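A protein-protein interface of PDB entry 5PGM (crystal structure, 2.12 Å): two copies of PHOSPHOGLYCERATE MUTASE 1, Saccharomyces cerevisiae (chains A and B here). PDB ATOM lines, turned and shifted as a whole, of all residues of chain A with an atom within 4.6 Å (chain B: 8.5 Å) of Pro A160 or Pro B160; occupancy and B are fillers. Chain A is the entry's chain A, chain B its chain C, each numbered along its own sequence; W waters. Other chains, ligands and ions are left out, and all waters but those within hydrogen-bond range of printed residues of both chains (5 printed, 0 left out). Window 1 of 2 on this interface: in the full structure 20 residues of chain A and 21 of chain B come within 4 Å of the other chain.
NH2 of Arg A83 touches CA of Pro B160, at 3.8 Å.
Pro A160 touches Arg B83 (CA to NH2, 3.9 Å).
Pro B160 touches Pro A160.
Asp B141 touches Trp A162.
Gln A163 touches Val B140 (O to CA, 3.8 Å).
Gln A163 touches Val B144.
Hydrophobic or aromatic side chains of chain B within 4 Å of the printed part of chain A: Trp B82, Val B140, Val B144 and Pro B160.
Of the 11 printed residues of chain A, 5 touch a printed residue of chain B.
Hydrophobic or aromatic side chains of chain A that line the printed part of chain B: Pro A160 and Trp A162.
Among the printed residues, Asp or Glu carboxylates within 4 Å of a Lys or Arg side-chain nitrogen of the other chain: Arg A83 with Asp B164 (2.6 Å) and Asp A164 with Arg B83 (2.6 Å).
Arg A83 touches Pro B160, and with the chains exchanged Pro A160 touches Arg B83.
Arg A83 touches Gln B163, and with the chains exchanged Gln A163 touches Arg B83.
Arg A83 touches Asp B164, and with the chains exchanged Asp A164 touches Arg B83.
Pro A160 touches its own counterpart, Pro B160.
11 positions are printed for both chains.
NH1 of Arg B83 sits at hydrogen-bond distance from O of Arg B157 (2.7 Å).
The side-chain amide oxygen (OE1) of Gln A163 lies close to the backbone carbonyl oxygen (O) of Leu A159, at 3.4 Å.
The side-chain hydroxyl of Ser B81 lies close to the backbone NH of Arg B83.
The guanidinium group of Arg A83 lies within hydrogen-bond range of the backbone carbonyl oxygen of Arg A157, 2.8 Å away.
O of Leu B159 sits close to OE1 of Gln B163, 3.3 Å away.
Printed residues of chain B within 4 Å of Arg A83: Pro B160, Gln B163 and Asp B164.
Of chain B, only Arg B83 and Pro B160 come within 4 Å of Pro A160.
Of the printed residues of chain B, Trp A162 touches Asp B141 (3.9 Å).
Of the printed residues of chain B, Gln A163 touches Arg B83 (2.9 Å), Val B140 (3.8 Å), Asp B141 (3.0 Å) and Val B144 (3.6 Å).
Printed residues of chain A within 4 Å of Arg B83: Pro A160, Gln A163 and Asp A164.
Leu B159 touches none of the printed residues of chain A.
Of chain A, only Arg A83 (3.8 Å) and Pro A160 (3.4 Å) come within 4 Å of Pro B160.
Printed residues of chain A within 4 Å of Gln B163: Arg A83 (3.2 Å).
Val B165 touches none of the printed residues of chain A.
The nearest residue of chain B that does not touch Pro A160 is Asp B156 (5.8 Å).
The nearest printed residue of chain A that does not touch Pro B160 is Asp A156 (5.8 Å).
The nearest printed residue of chain A that does not touch Val B140 is Asp A164 (4.1 Å).
The side-chain carboxylate (OD2) of Asp B164 is in salt-bridge range of the guanidinium group (NE) of Arg A83.
The guanidinium group (NH2) of Arg B83 sits at hydrogen-bond distance from the side-chain amide oxygen (OE1) of Gln A163 (2.9 Å).
OE1 of Gln B163 lies within hydrogen-bond range of NH2 of Arg A83, 3.2 Å away.
NE1 of Trp B82 lies within hydrogen-bond range of OD1 of Asp A164.
The backbone NH of Asp B141 is in hydrogen-bond range of the backbone carbonyl oxygen of Gln A163 (3.0 Å).
The side-chain carboxylate (OD2) of Asp A164 lies within salt-bridge range of the guanidinium group (NE) of Arg B83, at 2.6 Å.
Water W3 lies within hydrogen-bond range of NE2 of Gln A163 (2.6 Å) and OD2 of Asp B141 (2.7 Å).
Water W5 bridges NH1 of Arg B83 (2.8 Å) and OE1 of Gln A163 (2.8 Å).
Water W1 bridges OD2 of Asp B141 (2.9 Å) and NE1 of Trp A162 (3.1 Å).
Water W2 lies within hydrogen-bond range of the side-chain hydroxyl (OG) of Ser B81 and the side-chain carboxylate (OD2) of Asp A164.
Water W4 lies within hydrogen-bond range of OE1 of Gln B163 (3.0 Å) and NH1 of Arg A83 (3.1 Å).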
ATOM      1  N   ARG A  83     -32.323 -29.711 -34.664  1.00  0.00           N
ATOM      2  CA  ARG A  83     -31.026 -29.134 -35.006  1.00  0.00           C
ATOM      3  C   ARG A  83     -30.255 -29.962 -35.970  1.00  0.00           C
ATOM      4  O   ARG A  83     -29.232 -29.500 -36.456  1.00  0.00           O
ATOM      5  CB  ARG A  83     -30.180 -28.810 -33.753  1.00  0.00           C
ATOM      6  CG  ARG A  83     -30.825 -27.747 -32.853  1.00  0.00           C
ATOM      7  CD  ARG A  83     -29.969 -27.349 -31.591  1.00  0.00           C
ATOM      8  NE  ARG A  83     -30.767 -26.382 -30.834  1.00  0.00           N
ATOM      9  CZ  ARG A  83     -30.633 -25.055 -30.918  1.00  0.00           C
ATOM     10  NH1 ARG A  83     -29.692 -24.526 -31.690  1.00  0.00           N
ATOM     11  NH2 ARG A  83     -31.555 -24.263 -30.379  1.00  0.00           N
ATOM     12  N   ASP A 156     -25.171 -22.773 -37.522  1.00  0.00           N
ATOM     13  CA  ASP A 156     -25.384 -22.012 -36.306  1.00  0.00           C
ATOM     14  C   ASP A 156     -26.350 -22.700 -35.345  1.00  0.00           C
ATOM     15  O   ASP A 156     -26.147 -22.683 -34.121  1.00  0.00           O
ATOM     16  CB  ASP A 156     -25.881 -20.589 -36.573  1.00  0.00           C
ATOM     17  CG  ASP A 156     -24.801 -19.653 -37.167  1.00  0.00           C
ATOM     18  OD1 ASP A 156     -23.572 -19.912 -37.086  1.00  0.00           O
ATOM     19  OD2 ASP A 156     -25.215 -18.618 -37.723  1.00  0.00           O
ATOM     20  N   ARG A 157     -27.422 -23.265 -35.871  1.00  0.00           N
ATOM     21  CA  ARG A 157     -28.376 -23.951 -34.998  1.00  0.00           C
ATOM     22  C   ARG A 157     -27.999 -25.401 -34.685  1.00  0.00           C
ATOM     23  O   ARG A 157     -28.440 -25.958 -33.695  1.00  0.00           O
ATOM     24  CB  ARG A 157     -29.807 -23.810 -35.512  1.00  0.00           C
ATOM     25  CG  ARG A 157     -30.045 -24.114 -36.997  1.00  0.00           C
ATOM     26  CD  ARG A 157     -30.264 -25.587 -37.251  1.00  0.00           C
ATOM     27  NE  ARG A 157     -30.953 -25.830 -38.507  1.00  0.00           N
ATOM     28  CZ  ARG A 157     -30.935 -26.973 -39.187  1.00  0.00           C
ATOM     29  NH1 ARG A 157     -30.259 -28.010 -38.748  1.00  0.00           N
ATOM     30  NH2 ARG A 157     -31.603 -27.066 -40.322  1.00  0.00           N
ATOM     31  N   LEU A 158     -27.082 -25.971 -35.434  1.00  0.00           N
ATOM     32  CA  LEU A 158     -26.697 -27.347 -35.189  1.00  0.00           C
ATOM     33  C   LEU A 158     -25.589 -27.504 -34.159  1.00  0.00           C
ATOM     34  O   LEU A 158     -25.615 -28.425 -33.378  1.00  0.00           O
ATOM     35  CB  LEU A 158     -26.263 -28.023 -36.506  1.00  0.00           C
ATOM     36  CG  LEU A 158     -25.858 -29.513 -36.574  1.00  0.00           C
ATOM     37  CD1 LEU A 158     -26.162 -29.970 -37.977  1.00  0.00           C
ATOM     38  CD2 LEU A 158     -24.370 -29.782 -36.242  1.00  0.00           C
ATOM     39  N   LEU A 159     -24.587 -26.643 -34.212  1.00  0.00           N
ATOM     40  CA  LEU A 159     -23.463 -26.733 -33.330  1.00  0.00           C
ATOM     41  C   LEU A 159     -23.755 -26.844 -31.839  1.00  0.00           C
ATOM     42  O   LEU A 159     -23.070 -27.594 -31.142  1.00  0.00           O
ATOM     43  CB  LEU A 159     -22.467 -25.610 -33.612  1.00  0.00           C
ATOM     44  CG  LEU A 159     -21.588 -25.829 -34.848  1.00  0.00           C
ATOM     45  CD1 LEU A 159     -20.606 -24.703 -35.018  1.00  0.00           C
ATOM     46  CD2 LEU A 159     -20.838 -27.157 -34.668  1.00  0.00           C
ATOM     47  N   PRO A 160     -24.758 -26.126 -31.328  1.00  0.00           N
ATOM     48  CA  PRO A 160     -25.052 -26.220 -29.895  1.00  0.00           C
ATOM     49  C   PRO A 160     -25.389 -27.651 -29.472  1.00  0.00           C
ATOM     50  O   PRO A 160     -24.884 -28.131 -28.459  1.00  0.00           O
ATOM     51  CB  PRO A 160     -26.233 -25.248 -29.738  1.00  0.00           C
ATOM     52  CG  PRO A 160     -25.921 -24.204 -30.765  1.00  0.00           C
ATOM     53  CD  PRO A 160     -25.601 -25.099 -31.945  1.00  0.00           C
ATOM     54  N   TYR A 161     -26.147 -28.359 -30.320  1.00  0.00           N
ATOM     55  CA  TYR A 161     -26.532 -29.755 -30.062  1.00  0.00           C
ATOM     56  C   TYR A 161     -25.304 -30.631 -30.124  1.00  0.00           C
ATOM     57  O   TYR A 161     -25.145 -31.555 -29.334  1.00  0.00           O
ATOM     58  CB  TYR A 161     -27.543 -30.245 -31.103  1.00  0.00           C
ATOM     59  CG  TYR A 161     -28.232 -31.528 -30.725  1.00  0.00           C
ATOM     60  CD1 TYR A 161     -29.254 -31.532 -29.755  1.00  0.00           C
ATOM     61  CD2 TYR A 161     -27.877 -32.751 -31.329  1.00  0.00           C
ATOM     62  CE1 TYR A 161     -29.911 -32.726 -29.394  1.00  0.00           C
ATOM     63  CE2 TYR A 161     -28.537 -33.984 -30.955  1.00  0.00           C
ATOM     64  CZ  TYR A 161     -29.551 -33.939 -29.997  1.00  0.00           C
ATOM     65  OH  TYR A 161     -30.256 -35.059 -29.678  1.00  0.00           O
ATOM     66  N   TRP A 162     -24.445 -30.369 -31.095  1.00  0.00           N
ATOM     67  CA  TRP A 162     -23.246 -31.143 -31.228  1.00  0.00           C
ATOM     68  C   TRP A 162     -22.380 -30.932 -29.993  1.00  0.00           C
ATOM     69  O   TRP A 162     -21.807 -31.873 -29.443  1.00  0.00           O
ATOM     70  CB  TRP A 162     -22.495 -30.707 -32.479  1.00  0.00           C
ATOM     71  CG  TRP A 162     -21.036 -31.065 -32.521  1.00  0.00           C
ATOM     72  CD1 TRP A 162     -20.008 -30.240 -32.243  1.00  0.00           C
ATOM     73  CD2 TRP A 162     -20.451 -32.333 -32.858  1.00  0.00           C
ATOM     74  NE1 TRP A 162     -18.812 -30.908 -32.389  1.00  0.00           N
ATOM     75  CE2 TRP A 162     -19.069 -32.199 -32.758  1.00  0.00           C
ATOM     76  CE3 TRP A 162     -20.978 -33.598 -33.227  1.00  0.00           C
ATOM     77  CZ2 TRP A 162     -18.194 -33.260 -33.002  1.00  0.00           C
ATOM     78  CZ3 TRP A 162     -20.107 -34.634 -33.467  1.00  0.00           C
ATOM     79  CH2 TRP A 162     -18.735 -34.457 -33.355  1.00  0.00           C
ATOM     80  N   GLN A 163     -22.328 -29.679 -29.553  1.00  0.00           N
ATOM     81  CA  GLN A 163     -21.474 -29.261 -28.454  1.00  0.00           C
ATOM     82  C   GLN A 163     -21.745 -29.830 -27.093  1.00  0.00           C
ATOM     83  O   GLN A 163     -20.819 -30.150 -26.377  1.00  0.00           O
ATOM     84  CB  GLN A 163     -21.484 -27.733 -28.397  1.00  0.00           C
ATOM     85  CG  GLN A 163     -20.625 -27.151 -29.544  1.00  0.00           C
ATOM     86  CD  GLN A 163     -20.883 -25.660 -29.827  1.00  0.00           C
ATOM     87  OE1 GLN A 163     -21.856 -25.051 -29.315  1.00  0.00           O
ATOM     88  NE2 GLN A 163     -20.045 -25.086 -30.691  1.00  0.00           N
ATOM     89  N   ASP A 164     -23.023 -29.826 -26.729  1.00  0.00           N
ATOM     90  CA  ASP A 164     -23.514 -30.308 -25.458  1.00  0.00           C
ATOM     91  C   ASP A 164     -24.002 -31.760 -25.453  1.00  0.00           C
ATOM     92  O   ASP A 164     -23.637 -32.536 -24.581  1.00  0.00           O
ATOM     93  CB  ASP A 164     -24.673 -29.426 -24.970  1.00  0.00           C
ATOM     94  CG  ASP A 164     -24.222 -28.039 -24.554  1.00  0.00           C
ATOM     95  OD1 ASP A 164     -23.034 -27.720 -24.781  1.00  0.00           O
ATOM     96  OD2 ASP A 164     -25.069 -27.281 -24.037  1.00  0.00           O
ATOM     97  N   VAL A 165     -24.829 -32.119 -26.421  1.00  0.00           N
ATOM     98  CA  VAL A 165     -25.411 -33.455 -26.465  1.00  0.00           C
ATOM     99  C   VAL A 165     -24.627 -34.540 -27.167  1.00  0.00           C
ATOM    100  O   VAL A 165     -24.271 -35.547 -26.549  1.00  0.00           O
ATOM    101  CB  VAL A 165     -26.820 -33.378 -26.973  1.00  0.00           C
ATOM    102  CG1 VAL A 165     -27.545 -34.703 -26.762  1.00  0.00           C
ATOM    103  CG2 VAL A 165     -27.550 -32.219 -26.258  1.00  0.00           C
ATOM    104  N   SER B  81     -26.177 -26.131 -16.413  1.00  0.00           N
ATOM    105  CA  SER B  81     -25.565 -25.939 -17.723  1.00  0.00           C
ATOM    106  C   SER B  81     -24.522 -24.858 -17.700  1.00  0.00           C
ATOM    107  O   SER B  81     -24.744 -23.794 -17.149  1.00  0.00           O
ATOM    108  CB  SER B  81     -26.620 -25.520 -18.761  1.00  0.00           C
ATOM    109  OG  SER B  81     -25.965 -25.319 -20.017  1.00  0.00           O
ATOM    110  N   TRP B  82     -23.403 -25.116 -18.350  1.00  0.00           N
ATOM    111  CA  TRP B  82     -22.363 -24.117 -18.482  1.00  0.00           C
ATOM    112  C   TRP B  82     -22.929 -22.874 -19.240  1.00  0.00           C
ATOM    113  O   TRP B  82     -22.391 -21.776 -19.125  1.00  0.00           O
ATOM    114  CB  TRP B  82     -21.185 -24.689 -19.270  1.00  0.00           C
ATOM    115  CG  TRP B  82     -21.418 -24.805 -20.800  1.00  0.00           C
ATOM    116  CD1 TRP B  82     -21.920 -25.903 -21.502  1.00  0.00           C
ATOM    117  CD2 TRP B  82     -21.076 -23.825 -21.798  1.00  0.00           C
ATOM    118  NE1 TRP B  82     -21.892 -25.655 -22.851  1.00  0.00           N
ATOM    119  CE2 TRP B  82     -21.379 -24.402 -23.070  1.00  0.00           C
ATOM    120  CE3 TRP B  82     -20.536 -22.527 -21.742  1.00  0.00           C
ATOM    121  CZ2 TRP B  82     -21.147 -23.712 -24.285  1.00  0.00           C
ATOM    122  CZ3 TRP B  82     -20.307 -21.840 -22.945  1.00  0.00           C
ATOM    123  CH2 TRP B  82     -20.610 -22.435 -24.200  1.00  0.00           C
ATOM    124  N   ARG B  83     -24.002 -23.057 -20.016  1.00  0.00           N
ATOM    125  CA  ARG B  83     -24.576 -21.978 -20.802  1.00  0.00           C
ATOM    126  C   ARG B  83     -25.270 -20.934 -19.992  1.00  0.00           C
ATOM    127  O   ARG B  83     -25.626 -19.885 -20.515  1.00  0.00           O
ATOM    128  CB  ARG B  83     -25.479 -22.530 -21.914  1.00  0.00           C
ATOM    129  CG  ARG B  83     -24.686 -23.433 -22.873  1.00  0.00           C
ATOM    130  CD  ARG B  83     -25.532 -24.058 -24.020  1.00  0.00           C
ATOM    131  NE  ARG B  83     -24.651 -24.827 -24.896  1.00  0.00           N
ATOM    132  CZ  ARG B  83     -24.077 -24.362 -26.008  1.00  0.00           C
ATOM    133  NH1 ARG B  83     -24.304 -23.116 -26.400  1.00  0.00           N
ATOM    134  NH2 ARG B  83     -23.188 -25.106 -26.684  1.00  0.00           N
ATOM    135  N   VAL B 140     -18.276 -31.409 -22.280  1.00  0.00           N
ATOM    136  CA  VAL B 140     -18.651 -30.363 -23.224  1.00  0.00           C
ATOM    137  C   VAL B 140     -17.559 -30.366 -24.310  1.00  0.00           C
ATOM    138  O   VAL B 140     -16.430 -30.771 -24.061  1.00  0.00           O
ATOM    139  CB  VAL B 140     -18.716 -28.972 -22.546  1.00  0.00           C
ATOM    140  CG1 VAL B 140     -19.126 -27.882 -23.589  1.00  0.00           C
ATOM    141  CG2 VAL B 140     -19.723 -28.985 -21.416  1.00  0.00           C
ATOM    142  N   ASP B 141     -17.915 -30.018 -25.539  1.00  0.00           N
ATOM    143  CA  ASP B 141     -16.935 -29.979 -26.614  1.00  0.00           C
ATOM    144  C   ASP B 141     -15.881 -28.975 -26.135  1.00  0.00           C
ATOM    145  O   ASP B 141     -16.192 -27.823 -25.842  1.00  0.00           O
ATOM    146  CB  ASP B 141     -17.650 -29.481 -27.888  1.00  0.00           C
ATOM    147  CG  ASP B 141     -16.702 -29.106 -29.000  1.00  0.00           C
ATOM    148  OD1 ASP B 141     -15.514 -29.487 -29.049  1.00  0.00           O
ATOM    149  OD2 ASP B 141     -17.165 -28.378 -29.861  1.00  0.00           O
ATOM    150  N   VAL B 144     -15.765 -25.198 -27.809  1.00  0.00           N
ATOM    151  CA  VAL B 144     -16.729 -24.133 -27.588  1.00  0.00           C
ATOM    152  C   VAL B 144     -16.527 -23.358 -26.297  1.00  0.00           C
ATOM    153  O   VAL B 144     -17.047 -22.241 -26.141  1.00  0.00           O
ATOM    154  CB  VAL B 144     -18.131 -24.674 -27.560  1.00  0.00           C
ATOM    155  CG1 VAL B 144     -18.359 -25.504 -26.339  1.00  0.00           C
ATOM    156  CG2 VAL B 144     -19.098 -23.576 -27.552  1.00  0.00           C
ATOM    157  N   LEU B 153     -21.549 -12.522 -26.817  1.00  0.00           N
ATOM    158  CA  LEU B 153     -21.114 -13.904 -26.860  1.00  0.00           C
ATOM    159  C   LEU B 153     -21.845 -14.784 -25.792  1.00  0.00           C
ATOM    160  O   LEU B 153     -22.183 -15.938 -26.066  1.00  0.00           O
ATOM    161  CB  LEU B 153     -19.620 -13.893 -26.642  1.00  0.00           C
ATOM    162  CG  LEU B 153     -18.645 -14.343 -27.724  1.00  0.00           C
ATOM    163  CD1 LEU B 153     -19.261 -14.286 -29.087  1.00  0.00           C
ATOM    164  CD2 LEU B 153     -17.392 -13.554 -27.638  1.00  0.00           C
ATOM    165  N   VAL B 154     -22.099 -14.238 -24.595  1.00  0.00           N
ATOM    166  CA  VAL B 154     -22.810 -14.964 -23.530  1.00  0.00           C
ATOM    167  C   VAL B 154     -24.168 -15.334 -24.057  1.00  0.00           C
ATOM    168  O   VAL B 154     -24.586 -16.467 -23.974  1.00  0.00           O
ATOM    169  CB  VAL B 154     -22.988 -14.107 -22.239  1.00  0.00           C
ATOM    170  CG1 VAL B 154     -24.136 -14.614 -21.337  1.00  0.00           C
ATOM    171  CG2 VAL B 154     -21.701 -14.123 -21.452  1.00  0.00           C
ATOM    172  N   ILE B 155     -24.853 -14.354 -24.615  1.00  0.00           N
ATOM    173  CA  ILE B 155     -26.185 -14.535 -25.163  1.00  0.00           C
ATOM    174  C   ILE B 155     -26.164 -15.603 -26.269  1.00  0.00           C
ATOM    175  O   ILE B 155     -27.069 -16.429 -26.345  1.00  0.00           O
ATOM    176  CB  ILE B 155     -26.710 -13.185 -25.733  1.00  0.00           C
ATOM    177  CG1 ILE B 155     -26.736 -12.125 -24.613  1.00  0.00           C
ATOM    178  CG2 ILE B 155     -28.115 -13.363 -26.353  1.00  0.00           C
ATOM    179  CD1 ILE B 155     -27.345 -10.841 -25.011  1.00  0.00           C
ATOM    180  N   ASP B 156     -25.104 -15.610 -27.084  1.00  0.00           N
ATOM    181  CA  ASP B 156     -24.987 -16.580 -28.173  1.00  0.00           C
ATOM    182  C   ASP B 156     -24.893 -18.041 -27.661  1.00  0.00           C
ATOM    183  O   ASP B 156     -25.461 -18.954 -28.291  1.00  0.00           O
ATOM    184  CB  ASP B 156     -23.776 -16.288 -29.091  1.00  0.00           C
ATOM    185  CG  ASP B 156     -23.995 -15.117 -30.078  1.00  0.00           C
ATOM    186  OD1 ASP B 156     -25.112 -14.552 -30.242  1.00  0.00           O
ATOM    187  OD2 ASP B 156     -22.978 -14.769 -30.712  1.00  0.00           O
ATOM    188  N   ARG B 157     -24.196 -18.276 -26.547  1.00  0.00           N
ATOM    189  CA  ARG B 157     -24.075 -19.637 -26.033  1.00  0.00           C
ATOM    190  C   ARG B 157     -25.202 -20.013 -25.080  1.00  0.00           C
ATOM    191  O   ARG B 157     -25.503 -21.187 -24.913  1.00  0.00           O
ATOM    192  CB  ARG B 157     -22.688 -19.951 -25.516  1.00  0.00           C
ATOM    193  CG  ARG B 157     -22.098 -18.999 -24.515  1.00  0.00           C
ATOM    194  CD  ARG B 157     -22.727 -19.106 -23.121  1.00  0.00           C
ATOM    195  NE  ARG B 157     -21.820 -18.494 -22.182  1.00  0.00           N
ATOM    196  CZ  ARG B 157     -22.092 -18.153 -20.927  1.00  0.00           C
ATOM    197  NH1 ARG B 157     -23.299 -18.350 -20.398  1.00  0.00           N
ATOM    198  NH2 ARG B 157     -21.137 -17.619 -20.205  1.00  0.00           N
ATOM    199  N   LEU B 158     -25.920 -19.003 -24.599  1.00  0.00           N
ATOM    200  CA  LEU B 158     -27.041 -19.206 -23.710  1.00  0.00           C
ATOM    201  C   LEU B 158     -28.306 -19.549 -24.459  1.00  0.00           C
ATOM    202  O   LEU B 158     -29.041 -20.456 -24.070  1.00  0.00           O
ATOM    203  CB  LEU B 158     -27.337 -17.930 -22.904  1.00  0.00           C
ATOM    204  CG  LEU B 158     -28.414 -18.040 -21.809  1.00  0.00           C
ATOM    205  CD1 LEU B 158     -28.016 -17.269 -20.564  1.00  0.00           C
ATOM    206  CD2 LEU B 158     -29.707 -17.519 -22.280  1.00  0.00           C
ATOM    207  N   LEU B 159     -28.613 -18.777 -25.501  1.00  0.00           N
ATOM    208  CA  LEU B 159     -29.862 -19.004 -26.239  1.00  0.00           C
ATOM    209  C   LEU B 159     -30.250 -20.453 -26.640  1.00  0.00           C
ATOM    210  O   LEU B 159     -31.410 -20.786 -26.575  1.00  0.00           O
ATOM    211  CB  LEU B 159     -29.987 -18.035 -27.435  1.00  0.00           C
ATOM    212  CG  LEU B 159     -30.216 -16.588 -27.027  1.00  0.00           C
ATOM    213  CD1 LEU B 159     -30.232 -15.712 -28.263  1.00  0.00           C
ATOM    214  CD2 LEU B 159     -31.535 -16.486 -26.324  1.00  0.00           C
ATOM    215  N   PRO B 160     -29.320 -21.264 -27.155  1.00  0.00           N
ATOM    216  CA  PRO B 160     -29.656 -22.649 -27.535  1.00  0.00           C
ATOM    217  C   PRO B 160     -30.255 -23.470 -26.367  1.00  0.00           C
ATOM    218  O   PRO B 160     -31.211 -24.227 -26.566  1.00  0.00           O
ATOM    219  CB  PRO B 160     -28.310 -23.225 -27.927  1.00  0.00           C
ATOM    220  CG  PRO B 160     -27.629 -22.096 -28.511  1.00  0.00           C
ATOM    221  CD  PRO B 160     -27.961 -20.938 -27.609  1.00  0.00           C
ATOM    222  N   TYR B 161     -29.709 -23.284 -25.155  1.00  0.00           N
ATOM    223  CA  TYR B 161     -30.179 -23.995 -23.981  1.00  0.00           C
ATOM    224  C   TYR B 161     -31.580 -23.556 -23.624  1.00  0.00           C
ATOM    225  O   TYR B 161     -32.441 -24.352 -23.243  1.00  0.00           O
ATOM    226  CB  TYR B 161     -29.187 -23.764 -22.824  1.00  0.00           C
ATOM    227  CG  TYR B 161     -29.394 -24.670 -21.641  1.00  0.00           C
ATOM    228  CD1 TYR B 161     -28.971 -26.004 -21.660  1.00  0.00           C
ATOM    229  CD2 TYR B 161     -30.049 -24.211 -20.517  1.00  0.00           C
ATOM    230  CE1 TYR B 161     -29.211 -26.831 -20.558  1.00  0.00           C
ATOM    231  CE2 TYR B 161     -30.295 -25.014 -19.447  1.00  0.00           C
ATOM    232  CZ  TYR B 161     -29.874 -26.320 -19.457  1.00  0.00           C
ATOM    233  OH  TYR B 161     -30.084 -27.085 -18.330  1.00  0.00           O
ATOM    234  N   TRP B 162     -31.805 -22.260 -23.758  1.00  0.00           N
ATOM    235  CA  TRP B 162     -33.095 -21.673 -23.473  1.00  0.00           C
ATOM    236  C   TRP B 162     -34.108 -22.198 -24.509  1.00  0.00           C
ATOM    237  O   TRP B 162     -35.241 -22.556 -24.190  1.00  0.00           O
ATOM    238  CB  TRP B 162     -32.967 -20.102 -23.569  1.00  0.00           C
ATOM    239  CG  TRP B 162     -34.284 -19.348 -23.718  1.00  0.00           C
ATOM    240  CD1 TRP B 162     -34.836 -18.883 -24.895  1.00  0.00           C
ATOM    241  CD2 TRP B 162     -35.267 -19.088 -22.695  1.00  0.00           C
ATOM    242  NE1 TRP B 162     -36.091 -18.398 -24.670  1.00  0.00           N
ATOM    243  CE2 TRP B 162     -36.378 -18.493 -23.331  1.00  0.00           C
ATOM    244  CE3 TRP B 162     -35.310 -19.296 -21.316  1.00  0.00           C
ATOM    245  CZ2 TRP B 162     -37.523 -18.095 -22.633  1.00  0.00           C
ATOM    246  CZ3 TRP B 162     -36.458 -18.902 -20.609  1.00  0.00           C
ATOM    247  CH2 TRP B 162     -37.549 -18.306 -21.277  1.00  0.00           C
ATOM    248  N   GLN B 163     -33.681 -22.211 -25.762  1.00  0.00           N
ATOM    249  CA  GLN B 163     -34.548 -22.582 -26.872  1.00  0.00           C
ATOM    250  C   GLN B 163     -35.059 -24.006 -26.850  1.00  0.00           C
ATOM    251  O   GLN B 163     -36.251 -24.253 -27.119  1.00  0.00           O
ATOM    252  CB  GLN B 163     -33.828 -22.263 -28.219  1.00  0.00           C
ATOM    253  CG  GLN B 163     -33.784 -20.762 -28.594  1.00  0.00           C
ATOM    254  CD  GLN B 163     -32.650 -20.362 -29.566  1.00  0.00           C
ATOM    255  OE1 GLN B 163     -31.715 -21.125 -29.816  1.00  0.00           O
ATOM    256  NE2 GLN B 163     -32.715 -19.134 -30.064  1.00  0.00           N
ATOM    257  N   ASP B 164     -34.171 -24.927 -26.514  1.00  0.00           N
ATOM    258  CA  ASP B 164     -34.508 -26.355 -26.499  1.00  0.00           C
ATOM    259  C   ASP B 164     -34.822 -26.922 -25.122  1.00  0.00           C
ATOM    260  O   ASP B 164     -35.797 -27.641 -24.963  1.00  0.00           O
ATOM    261  CB  ASP B 164     -33.352 -27.193 -27.053  1.00  0.00           C
ATOM    262  CG  ASP B 164     -33.117 -26.995 -28.538  1.00  0.00           C
ATOM    263  OD1 ASP B 164     -33.827 -26.181 -29.196  1.00  0.00           O
ATOM    264  OD2 ASP B 164     -32.199 -27.682 -29.046  1.00  0.00           O
ATOM    265  N   VAL B 165     -33.951 -26.653 -24.152  1.00  0.00           N
ATOM    266  CA  VAL B 165     -34.136 -27.220 -22.842  1.00  0.00           C
ATOM    267  C   VAL B 165     -35.111 -26.518 -21.940  1.00  0.00           C
ATOM    268  O   VAL B 165     -36.125 -27.090 -21.575  1.00  0.00           O
ATOM    269  CB  VAL B 165     -32.782 -27.477 -22.166  1.00  0.00           C
ATOM    270  CG1 VAL B 165     -32.964 -28.197 -20.831  1.00  0.00           C
ATOM    271  CG2 VAL B 165     -31.858 -28.269 -23.129  1.00  0.00           C
ATOM    272  N   ILE B 166     -34.864 -25.250 -21.632  1.00  0.00           N
ATOM    273  CA  ILE B 166     -35.743 -24.519 -20.744  1.00  0.00           C
ATOM    274  C   ILE B 166     -37.112 -24.309 -21.328  1.00  0.00           C
ATOM    275  O   ILE B 166     -38.111 -24.404 -20.621  1.00  0.00           O
ATOM    276  CB  ILE B 166     -35.065 -23.147 -20.321  1.00  0.00           C
ATOM    277  CG1 ILE B 166     -33.719 -23.436 -19.667  1.00  0.00           C
ATOM    278  CG2 ILE B 166     -35.973 -22.346 -19.385  1.00  0.00           C
ATOM    279  CD1 ILE B 166     -32.939 -22.193 -19.252  1.00  0.00           C
ATOM    280  N   ALA B 167     -37.163 -24.014 -22.628  1.00  0.00           N
ATOM    281  CA  ALA B 167     -38.449 -23.809 -23.334  1.00  0.00           C
ATOM    282  C   ALA B 167     -39.398 -25.014 -23.205  1.00  0.00           C
ATOM    283  O   ALA B 167     -40.614 -24.866 -23.063  1.00  0.00           O
ATOM    284  CB  ALA B 167     -38.201 -23.542 -24.794  1.00  0.00           C
ATOM    285  N   HIS B 191     -32.999 -10.631 -24.373  1.00  0.00           N
ATOM    286  CA  HIS B 191     -33.766 -11.450 -25.312  1.00  0.00           C
ATOM    287  C   HIS B 191     -35.281 -11.395 -25.046  1.00  0.00           C
ATOM    288  O   HIS B 191     -36.083 -11.144 -25.952  1.00  0.00           O
ATOM    289  CB  HIS B 191     -33.300 -12.920 -25.270  1.00  0.00           C
ATOM    290  CG  HIS B 191     -34.114 -13.833 -26.141  1.00  0.00           C
ATOM    291  ND1 HIS B 191     -33.663 -14.290 -27.356  1.00  0.00           N
ATOM    292  CD2 HIS B 191     -35.395 -14.275 -26.029  1.00  0.00           C
ATOM    293  CE1 HIS B 191     -34.626 -14.954 -27.960  1.00  0.00           C
ATOM    294  NE2 HIS B 191     -35.692 -14.962 -27.174  1.00  0.00           N
HETATM  295  O   HOH W   1     -16.079 -29.550 -32.225  1.00  0.00           O
HETATM  296  O   HOH W   2     -25.397 -27.850 -21.220  1.00  0.00           O
HETATM  297  O   HOH W   3     -17.843 -26.273 -31.434  1.00  0.00           O
HETATM  298  O   HOH W   4     -29.787 -21.485 -32.023  1.00  0.00           O
HETATM  299  O   HOH W   5     -22.750 -22.456 -28.655  1.00  0.00           O
